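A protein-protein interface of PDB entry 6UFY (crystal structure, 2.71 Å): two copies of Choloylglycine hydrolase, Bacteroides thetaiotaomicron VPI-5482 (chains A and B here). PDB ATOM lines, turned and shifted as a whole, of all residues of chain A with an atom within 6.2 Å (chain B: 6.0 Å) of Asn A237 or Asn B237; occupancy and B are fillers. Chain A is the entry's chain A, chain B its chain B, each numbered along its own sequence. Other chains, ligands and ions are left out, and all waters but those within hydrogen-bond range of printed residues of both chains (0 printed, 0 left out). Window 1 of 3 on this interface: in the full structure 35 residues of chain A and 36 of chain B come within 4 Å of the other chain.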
ATOM      1  N   GLY A 200      26.436  31.517 -27.906  1.00  0.00           N
ATOM      2  CA  GLY A 200      25.847  31.335 -26.594  1.00  0.00           C
ATOM      3  C   GLY A 200      24.405  30.873 -26.591  1.00  0.00           C
ATOM      4  O   GLY A 200      23.688  31.078 -25.607  1.00  0.00           O
ATOM      5  N   ARG A 210      31.287  25.894 -26.653  1.00  0.00           N
ATOM      6  CA  ARG A 210      31.493  26.514 -25.347  1.00  0.00           C
ATOM      7  C   ARG A 210      32.115  25.531 -24.365  1.00  0.00           C
ATOM      8  O   ARG A 210      33.002  25.897 -23.585  1.00  0.00           O
ATOM      9  CB  ARG A 210      30.173  27.054 -24.798  1.00  0.00           C
ATOM     10  CG  ARG A 210      29.550  28.155 -25.639  1.00  0.00           C
ATOM     11  CD  ARG A 210      28.678  29.067 -24.791  1.00  0.00           C
ATOM     12  NE  ARG A 210      27.770  28.317 -23.928  1.00  0.00           N
ATOM     13  CZ  ARG A 210      26.550  27.932 -24.281  1.00  0.00           C
ATOM     14  NH1 ARG A 210      25.793  27.256 -23.428  1.00  0.00           N
ATOM     15  NH2 ARG A 210      26.084  28.221 -25.489  1.00  0.00           N
ATOM     16  N   ALA A 211      31.662  24.275 -24.389  1.00  0.00           N
ATOM     17  CA  ALA A 211      32.251  23.263 -23.519  1.00  0.00           C
ATOM     18  C   ALA A 211      33.672  22.927 -23.948  1.00  0.00           C
ATOM     19  O   ALA A 211      34.542  22.692 -23.101  1.00  0.00           O
ATOM     20  CB  ALA A 211      31.383  22.005 -23.509  1.00  0.00           C
ATOM     21  N   TYR A 214      35.961  26.000 -22.824  1.00  0.00           N
ATOM     22  CA  TYR A 214      36.090  26.222 -21.388  1.00  0.00           C
ATOM     23  C   TYR A 214      36.757  25.051 -20.677  1.00  0.00           C
ATOM     24  O   TYR A 214      37.423  25.252 -19.656  1.00  0.00           O
ATOM     25  CB  TYR A 214      34.717  26.501 -20.775  1.00  0.00           C
ATOM     26  CG  TYR A 214      34.224  27.911 -20.996  1.00  0.00           C
ATOM     27  CD1 TYR A 214      35.112  28.977 -21.058  1.00  0.00           C
ATOM     28  CD2 TYR A 214      32.869  28.177 -21.146  1.00  0.00           C
ATOM     29  CE1 TYR A 214      34.664  30.267 -21.260  1.00  0.00           C
ATOM     30  CE2 TYR A 214      32.412  29.463 -21.348  1.00  0.00           C
ATOM     31  CZ  TYR A 214      33.313  30.505 -21.404  1.00  0.00           C
ATOM     32  OH  TYR A 214      32.860  31.788 -21.606  1.00  0.00           O
ATOM     33  N   LEU A 232      32.306  21.223 -12.985  1.00  0.00           N
ATOM     34  CA  LEU A 232      30.885  21.486 -12.803  1.00  0.00           C
ATOM     35  C   LEU A 232      30.519  22.874 -13.315  1.00  0.00           C
ATOM     36  O   LEU A 232      29.439  23.067 -13.881  1.00  0.00           O
ATOM     37  CB  LEU A 232      30.508  21.334 -11.328  1.00  0.00           C
ATOM     38  CG  LEU A 232      29.013  21.358 -10.999  1.00  0.00           C
ATOM     39  CD1 LEU A 232      28.310  20.127 -11.550  1.00  0.00           C
ATOM     40  CD2 LEU A 232      28.798  21.470  -9.500  1.00  0.00           C
ATOM     41  N   SER A 233      31.420  23.847 -13.146  1.00  0.00           N
ATOM     42  CA  SER A 233      31.128  25.214 -13.572  1.00  0.00           C
ATOM     43  C   SER A 233      30.907  25.292 -15.077  1.00  0.00           C
ATOM     44  O   SER A 233      29.981  25.969 -15.541  1.00  0.00           O
ATOM     45  CB  SER A 233      32.258  26.152 -13.151  1.00  0.00           C
ATOM     46  OG  SER A 233      33.422  25.927 -13.926  1.00  0.00           O
ATOM     47  N   VAL A 234      31.748  24.610 -15.861  1.00  0.00           N
ATOM     48  CA  VAL A 234      31.554  24.607 -17.305  1.00  0.00           C
ATOM     49  C   VAL A 234      30.334  23.786 -17.696  1.00  0.00           C
ATOM     50  O   VAL A 234      29.791  23.974 -18.789  1.00  0.00           O
ATOM     51  CB  VAL A 234      32.816  24.104 -18.035  1.00  0.00           C
ATOM     52  CG1 VAL A 234      34.053  24.829 -17.526  1.00  0.00           C
ATOM     53  CG2 VAL A 234      32.970  22.601 -17.888  1.00  0.00           C
ATOM     54  N   MET A 235      29.882  22.878 -16.824  1.00  0.00           N
ATOM     55  CA  MET A 235      28.635  22.166 -17.084  1.00  0.00           C
ATOM     56  C   MET A 235      27.436  23.099 -16.965  1.00  0.00           C
ATOM     57  O   MET A 235      26.510  23.038 -17.781  1.00  0.00           O
ATOM     58  CB  MET A 235      28.484  20.985 -16.126  1.00  0.00           C
ATOM     59  CG  MET A 235      29.399  19.814 -16.423  1.00  0.00           C
ATOM     60  SD  MET A 235      29.246  19.246 -18.125  1.00  0.00           S
ATOM     61  CE  MET A 235      30.827  19.764 -18.781  1.00  0.00           C
ATOM     62  N   ARG A 236      27.436  23.965 -15.949  1.00  0.00           N
ATOM     63  CA  ARG A 236      26.336  24.908 -15.788  1.00  0.00           C
ATOM     64  C   ARG A 236      26.362  25.983 -16.865  1.00  0.00           C
ATOM     65  O   ARG A 236      25.312  26.534 -17.216  1.00  0.00           O
ATOM     66  CB  ARG A 236      26.388  25.540 -14.398  1.00  0.00           C
ATOM     67  CG  ARG A 236      26.836  24.590 -13.299  1.00  0.00           C
ATOM     68  CD  ARG A 236      26.590  25.191 -11.932  1.00  0.00           C
ATOM     69  NE  ARG A 236      27.503  24.697 -10.908  1.00  0.00           N
ATOM     70  CZ  ARG A 236      27.448  25.065  -9.632  1.00  0.00           C
ATOM     71  NH1 ARG A 236      26.521  25.924  -9.230  1.00  0.00           N
ATOM     72  NH2 ARG A 236      28.315  24.580  -8.756  1.00  0.00           N
ATOM     73  N   ASN A 237      27.547  26.296 -17.398  1.00  0.00           N
ATOM     74  CA  ASN A 237      27.635  27.228 -18.516  1.00  0.00           C
ATOM     75  C   ASN A 237      26.942  26.661 -19.748  1.00  0.00           C
ATOM     76  O   ASN A 237      26.128  27.337 -20.386  1.00  0.00           O
ATOM     77  CB  ASN A 237      29.100  27.547 -18.819  1.00  0.00           C
ATOM     78  CG  ASN A 237      29.256  28.573 -19.927  1.00  0.00           C
ATOM     79  OD1 ASN A 237      29.332  28.226 -21.106  1.00  0.00           O
ATOM     80  ND2 ASN A 237      29.306  29.845 -19.549  1.00  0.00           N
ATOM     81  N   VAL A 238      27.258  25.409 -20.097  1.00  0.00           N
ATOM     82  CA  VAL A 238      26.607  24.751 -21.228  1.00  0.00           C
ATOM     83  C   VAL A 238      25.238  24.202 -20.873  1.00  0.00           C
ATOM     84  O   VAL A 238      24.572  23.620 -21.739  1.00  0.00           O
ATOM     85  CB  VAL A 238      27.487  23.615 -21.787  1.00  0.00           C
ATOM     86  CG1 VAL A 238      28.825  24.168 -22.241  1.00  0.00           C
ATOM     87  CG2 VAL A 238      27.675  22.526 -20.745  1.00  0.00           C
ATOM     88  N   SER A 239      24.799  24.356 -19.628  1.00  0.00           N
ATOM     89  CA  SER A 239      23.431  24.014 -19.282  1.00  0.00           C
ATOM     90  C   SER A 239      22.475  25.062 -19.843  1.00  0.00           C
ATOM     91  O   SER A 239      22.865  26.183 -20.181  1.00  0.00           O
ATOM     92  CB  SER A 239      23.265  23.907 -17.766  1.00  0.00           C
ATOM     93  OG  SER A 239      24.112  22.908 -17.226  1.00  0.00           O
ATOM     94  N   VAL A 240      21.209  24.681 -19.951  1.00  0.00           N
ATOM     95  CA  VAL A 240      20.183  25.602 -20.429  1.00  0.00           C
ATOM     96  C   VAL A 240      19.282  25.952 -19.251  1.00  0.00           C
ATOM     97  O   VAL A 240      18.988  25.082 -18.416  1.00  0.00           O
ATOM     98  CB  VAL A 240      19.405  25.007 -21.615  1.00  0.00           C
ATOM     99  CG1 VAL A 240      20.375  24.547 -22.694  1.00  0.00           C
ATOM    100  CG2 VAL A 240      18.535  23.849 -21.176  1.00  0.00           C
ATOM    101  N   PRO A 241      18.862  27.211 -19.113  1.00  0.00           N
ATOM    102  CA  PRO A 241      18.049  27.595 -17.954  1.00  0.00           C
ATOM    103  C   PRO A 241      16.734  26.829 -17.909  1.00  0.00           C
ATOM    104  O   PRO A 241      16.270  26.266 -18.903  1.00  0.00           O
ATOM    105  CB  PRO A 241      17.818  29.096 -18.160  1.00  0.00           C
ATOM    106  CG  PRO A 241      18.963  29.535 -19.014  1.00  0.00           C
ATOM    107  CD  PRO A 241      19.247  28.375 -19.928  1.00  0.00           C
ATOM    108  N   GLY B 200      28.073  34.672 -26.340  1.00  0.00           N
ATOM    109  CA  GLY B 200      28.317  33.765 -25.229  1.00  0.00           C
ATOM    110  C   GLY B 200      29.683  33.819 -24.568  1.00  0.00           C
ATOM    111  O   GLY B 200      30.132  32.841 -23.965  1.00  0.00           O
ATOM    112  N   ARG B 210      22.456  37.713 -22.490  1.00  0.00           N
ATOM    113  CA  ARG B 210      21.987  36.394 -22.072  1.00  0.00           C
ATOM    114  C   ARG B 210      21.135  36.469 -20.812  1.00  0.00           C
ATOM    115  O   ARG B 210      20.172  35.707 -20.672  1.00  0.00           O
ATOM    116  CB  ARG B 210      23.172  35.455 -21.852  1.00  0.00           C
ATOM    117  CG  ARG B 210      24.110  35.349 -23.046  1.00  0.00           C
ATOM    118  CD  ARG B 210      24.933  34.071 -22.992  1.00  0.00           C
ATOM    119  NE  ARG B 210      25.620  33.901 -21.714  1.00  0.00           N
ATOM    120  CZ  ARG B 210      26.835  34.370 -21.449  1.00  0.00           C
ATOM    121  NH1 ARG B 210      27.381  34.162 -20.259  1.00  0.00           N
ATOM    122  NH2 ARG B 210      27.504  35.050 -22.369  1.00  0.00           N
ATOM    123  N   ALA B 211      21.464  37.375 -19.890  1.00  0.00           N
ATOM    124  CA  ALA B 211      20.656  37.517 -18.683  1.00  0.00           C
ATOM    125  C   ALA B 211      19.293  38.118 -18.998  1.00  0.00           C
ATOM    126  O   ALA B 211      18.276  37.685 -18.445  1.00  0.00           O
ATOM    127  CB  ALA B 211      21.388  38.374 -17.652  1.00  0.00           C
ATOM    128  N   TYR B 214      17.082  35.332 -21.038  1.00  0.00           N
ATOM    129  CA  TYR B 214      16.637  34.167 -20.277  1.00  0.00           C
ATOM    130  C   TYR B 214      15.704  34.549 -19.134  1.00  0.00           C
ATOM    131  O   TYR B 214      14.804  33.775 -18.791  1.00  0.00           O
ATOM    132  CB  TYR B 214      17.846  33.399 -19.739  1.00  0.00           C
ATOM    133  CG  TYR B 214      18.589  32.606 -20.791  1.00  0.00           C
ATOM    134  CD1 TYR B 214      17.904  31.930 -21.791  1.00  0.00           C
ATOM    135  CD2 TYR B 214      19.977  32.538 -20.785  1.00  0.00           C
ATOM    136  CE1 TYR B 214      18.579  31.204 -22.755  1.00  0.00           C
ATOM    137  CE2 TYR B 214      20.661  31.814 -21.747  1.00  0.00           C
ATOM    138  CZ  TYR B 214      19.956  31.149 -22.728  1.00  0.00           C
ATOM    139  OH  TYR B 214      20.627  30.426 -23.689  1.00  0.00           O
ATOM    140  N   LEU B 232      18.069  31.192 -10.572  1.00  0.00           N
ATOM    141  CA  LEU B 232      19.381  30.685 -10.196  1.00  0.00           C
ATOM    142  C   LEU B 232      20.049  29.981 -11.370  1.00  0.00           C
ATOM    143  O   LEU B 232      21.274  30.050 -11.521  1.00  0.00           O
ATOM    144  CB  LEU B 232      19.239  29.751  -8.992  1.00  0.00           C
ATOM    145  CG  LEU B 232      20.453  29.183  -8.254  1.00  0.00           C
ATOM    146  CD1 LEU B 232      20.812  27.822  -8.810  1.00  0.00           C
ATOM    147  CD2 LEU B 232      21.643  30.132  -8.309  1.00  0.00           C
ATOM    148  N   SER B 233      19.258  29.319 -12.218  1.00  0.00           N
ATOM    149  CA  SER B 233      19.807  28.727 -13.434  1.00  0.00           C
ATOM    150  C   SER B 233      20.257  29.796 -14.419  1.00  0.00           C
ATOM    151  O   SER B 233      21.204  29.574 -15.182  1.00  0.00           O
ATOM    152  CB  SER B 233      18.773  27.806 -14.085  1.00  0.00           C
ATOM    153  OG  SER B 233      17.684  28.547 -14.607  1.00  0.00           O
ATOM    154  N   VAL B 234      19.598  30.957 -14.418  1.00  0.00           N
ATOM    155  CA  VAL B 234      20.005  32.040 -15.307  1.00  0.00           C
ATOM    156  C   VAL B 234      21.321  32.648 -14.838  1.00  0.00           C
ATOM    157  O   VAL B 234      22.188  32.988 -15.653  1.00  0.00           O
ATOM    158  CB  VAL B 234      18.891  33.100 -15.403  1.00  0.00           C
ATOM    159  CG1 VAL B 234      19.305  34.227 -16.339  1.00  0.00           C
ATOM    160  CG2 VAL B 234      17.596  32.463 -15.878  1.00  0.00           C
ATOM    161  N   MET B 235      21.499  32.786 -13.522  1.00  0.00           N
ATOM    162  CA  MET B 235      22.741  33.351 -13.004  1.00  0.00           C
ATOM    163  C   MET B 235      23.932  32.444 -13.289  1.00  0.00           C
ATOM    164  O   MET B 235      25.050  32.934 -13.481  1.00  0.00           O
ATOM    165  CB  MET B 235      22.621  33.618 -11.503  1.00  0.00           C
ATOM    166  CG  MET B 235      21.447  34.506 -11.116  1.00  0.00           C
ATOM    167  SD  MET B 235      21.190  35.896 -12.240  1.00  0.00           S
ATOM    168  CE  MET B 235      22.695  36.834 -11.995  1.00  0.00           C
ATOM    169  N   ARG B 236      23.713  31.127 -13.326  1.00  0.00           N
ATOM    170  CA  ARG B 236      24.792  30.212 -13.680  1.00  0.00           C
ATOM    171  C   ARG B 236      25.130  30.296 -15.162  1.00  0.00           C
ATOM    172  O   ARG B 236      26.281  30.062 -15.549  1.00  0.00           O
ATOM    173  CB  ARG B 236      24.414  28.781 -13.301  1.00  0.00           C
ATOM    174  CG  ARG B 236      24.118  28.581 -11.823  1.00  0.00           C
ATOM    175  CD  ARG B 236      23.779  27.132 -11.540  1.00  0.00           C
ATOM    176  NE  ARG B 236      23.542  26.879 -10.123  1.00  0.00           N
ATOM    177  CZ  ARG B 236      23.440  25.668  -9.588  1.00  0.00           C
ATOM    178  NH1 ARG B 236      23.572  24.591 -10.353  1.00  0.00           N
ATOM    179  NH2 ARG B 236      23.217  25.529  -8.289  1.00  0.00           N
ATOM    180  N   ASN B 237      24.147  30.630 -16.002  1.00  0.00           N
ATOM    181  CA  ASN B 237      24.415  30.775 -17.430  1.00  0.00           C
ATOM    182  C   ASN B 237      25.261  32.006 -17.714  1.00  0.00           C
ATOM    183  O   ASN B 237      26.119  31.981 -18.604  1.00  0.00           O
ATOM    184  CB  ASN B 237      23.099  30.841 -18.210  1.00  0.00           C
ATOM    185  CG  ASN B 237      23.322  30.957 -19.706  1.00  0.00           C
ATOM    186  OD1 ASN B 237      23.435  32.058 -20.241  1.00  0.00           O
ATOM    187  ND2 ASN B 237      23.406  29.817 -20.387  1.00  0.00           N
ATOM    188  N   VAL B 238      25.034  33.090 -16.972  1.00  0.00           N
ATOM    189  CA  VAL B 238      25.838  34.303 -17.094  1.00  0.00           C
ATOM    190  C   VAL B 238      27.041  34.284 -16.156  1.00  0.00           C
ATOM    191  O   VAL B 238      27.706  35.308 -16.000  1.00  0.00           O
ATOM    192  CB  VAL B 238      24.980  35.563 -16.859  1.00  0.00           C
ATOM    193  CG1 VAL B 238      23.873  35.668 -17.909  1.00  0.00           C
ATOM    194  CG2 VAL B 238      24.377  35.555 -15.469  1.00  0.00           C
ATOM    195  N   SER B 239      27.331  33.148 -15.522  1.00  0.00           N
ATOM    196  CA  SER B 239      28.524  33.053 -14.703  1.00  0.00           C
ATOM    197  C   SER B 239      29.756  32.778 -15.563  1.00  0.00           C
ATOM    198  O   SER B 239      29.663  32.332 -16.709  1.00  0.00           O
ATOM    199  CB  SER B 239      28.388  31.947 -13.651  1.00  0.00           C
ATOM    200  OG  SER B 239      27.495  32.302 -12.608  1.00  0.00           O
ATOM    201  N   VAL B 240      30.922  33.032 -14.986  1.00  0.00           N
ATOM    202  CA  VAL B 240      32.205  32.771 -15.637  1.00  0.00           C
ATOM    203  C   VAL B 240      32.794  31.502 -15.030  1.00  0.00           C
ATOM    204  O   VAL B 240      32.875  31.402 -13.796  1.00  0.00           O
ATOM    205  CB  VAL B 240      33.173  33.961 -15.480  1.00  0.00           C
ATOM    206  CG1 VAL B 240      34.507  33.679 -16.189  1.00  0.00           C
ATOM    207  CG2 VAL B 240      32.544  35.227 -16.030  1.00  0.00           C
ATOM    208  N   PRO B 241      33.195  30.517 -15.842  1.00  0.00           N
ATOM    209  CA  PRO B 241      33.754  29.285 -15.275  1.00  0.00           C
ATOM    210  C   PRO B 241      34.953  29.581 -14.388  1.00  0.00           C
ATOM    211  O   PRO B 241      35.649  30.584 -14.559  1.00  0.00           O
ATOM    212  CB  PRO B 241      34.149  28.469 -16.511  1.00  0.00           C
ATOM    213  CG  PRO B 241      33.250  28.970 -17.592  1.00  0.00           C
ATOM    214  CD  PRO B 241      33.056  30.439 -17.308  1.00  0.00           C
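The guanidinium group of Arg A236 lies close to the guanidinium group of Arg B236 (3.3 Å).
The backbone carbonyl oxygen of Asn B237 lies within hydrogen-bond range of the guanidinium group of Arg B210. The side-chain hydroxyl (OG) of Ser A239 sits at hydrogen-bond distance from the backbone carbonyl oxygen (O) of Met A235, 2.5 Å away. NH1 of Arg A210 lies within hydrogen-bond range of O of Asn A237 (3.1 Å). The backbone carbonyl oxygen of Met B235 lies within hydrogen-bond range of the side-chain hydroxyl of Ser B239.
Among the printed residues, pairs that only touch across the chains: Gly A200 with Gly B200 (3.7 Å), Gly A200 with Tyr B214 (3.7 Å), Tyr A214 with Gly B200 (3.8 Å), Tyr A214 with Pro B241 (3.7 Å), Ser A233 with Pro B241 (3.6 Å), Val A234 with Pro B241 (3.8 Å), Asn A237 with Asn B237 (3.7 Å), Asn A237 with Ser B239 (3.8 Å), Ser A239 with Asn B237 (3.7 Å), Pro A241 with Tyr B214 (3.6 Å) and Pro A241 with Ser B233 (3.5 Å).
Printed residues of chain B within 4 Å of Arg A236: Arg B236. Of the printed residues of chain B, Asn A237 touches Asn B237 (3.7 Å) and Ser B239 (3.8 Å). Of the printed residues of chain B, Ser A239 touches Asn B237. Of the printed residues of chain A, Gly B200 touches Gly A200 and Tyr A214. Of the printed residues of chain A, Asn B237 touches Asn A237 and Ser A239. Printed residues of chain A within 4 Å of Ser B239: Asn A237. The nearest residue of chain A that does not touch Asn B237 is Arg A236 (4.3 Å).
Hydrophobic or aromatic side chains of chain B within 4 Å of the printed part of chain A: Tyr B214 and Pro B241. Of the 14 printed residues of chain A, 8 touch a printed residue of chain B. Printed residues of chain A that touch a printed residue of chain B: Gly A200, Tyr A214, Ser A233, Val A234, Arg A236, Asn A237, Ser A239 and Pro A241. Hydrophobic or aromatic side chains of chain A that line the printed part of chain B: Tyr A214, Val A234 and Pro A241.
Gly B200 touches its own counterpart, Gly A200. Val A234 touches Pro B241, but with the chains exchanged Pro A241 does not touch Val B234 (4.1 Å). Arg A236 touches its own counterpart, Arg B236. Asn B237 touches its own counterpart, Asn A237. Of the 12 pairs that touch across the chains among the printed residues, 11 have their exchanged pair printed and touching as well.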
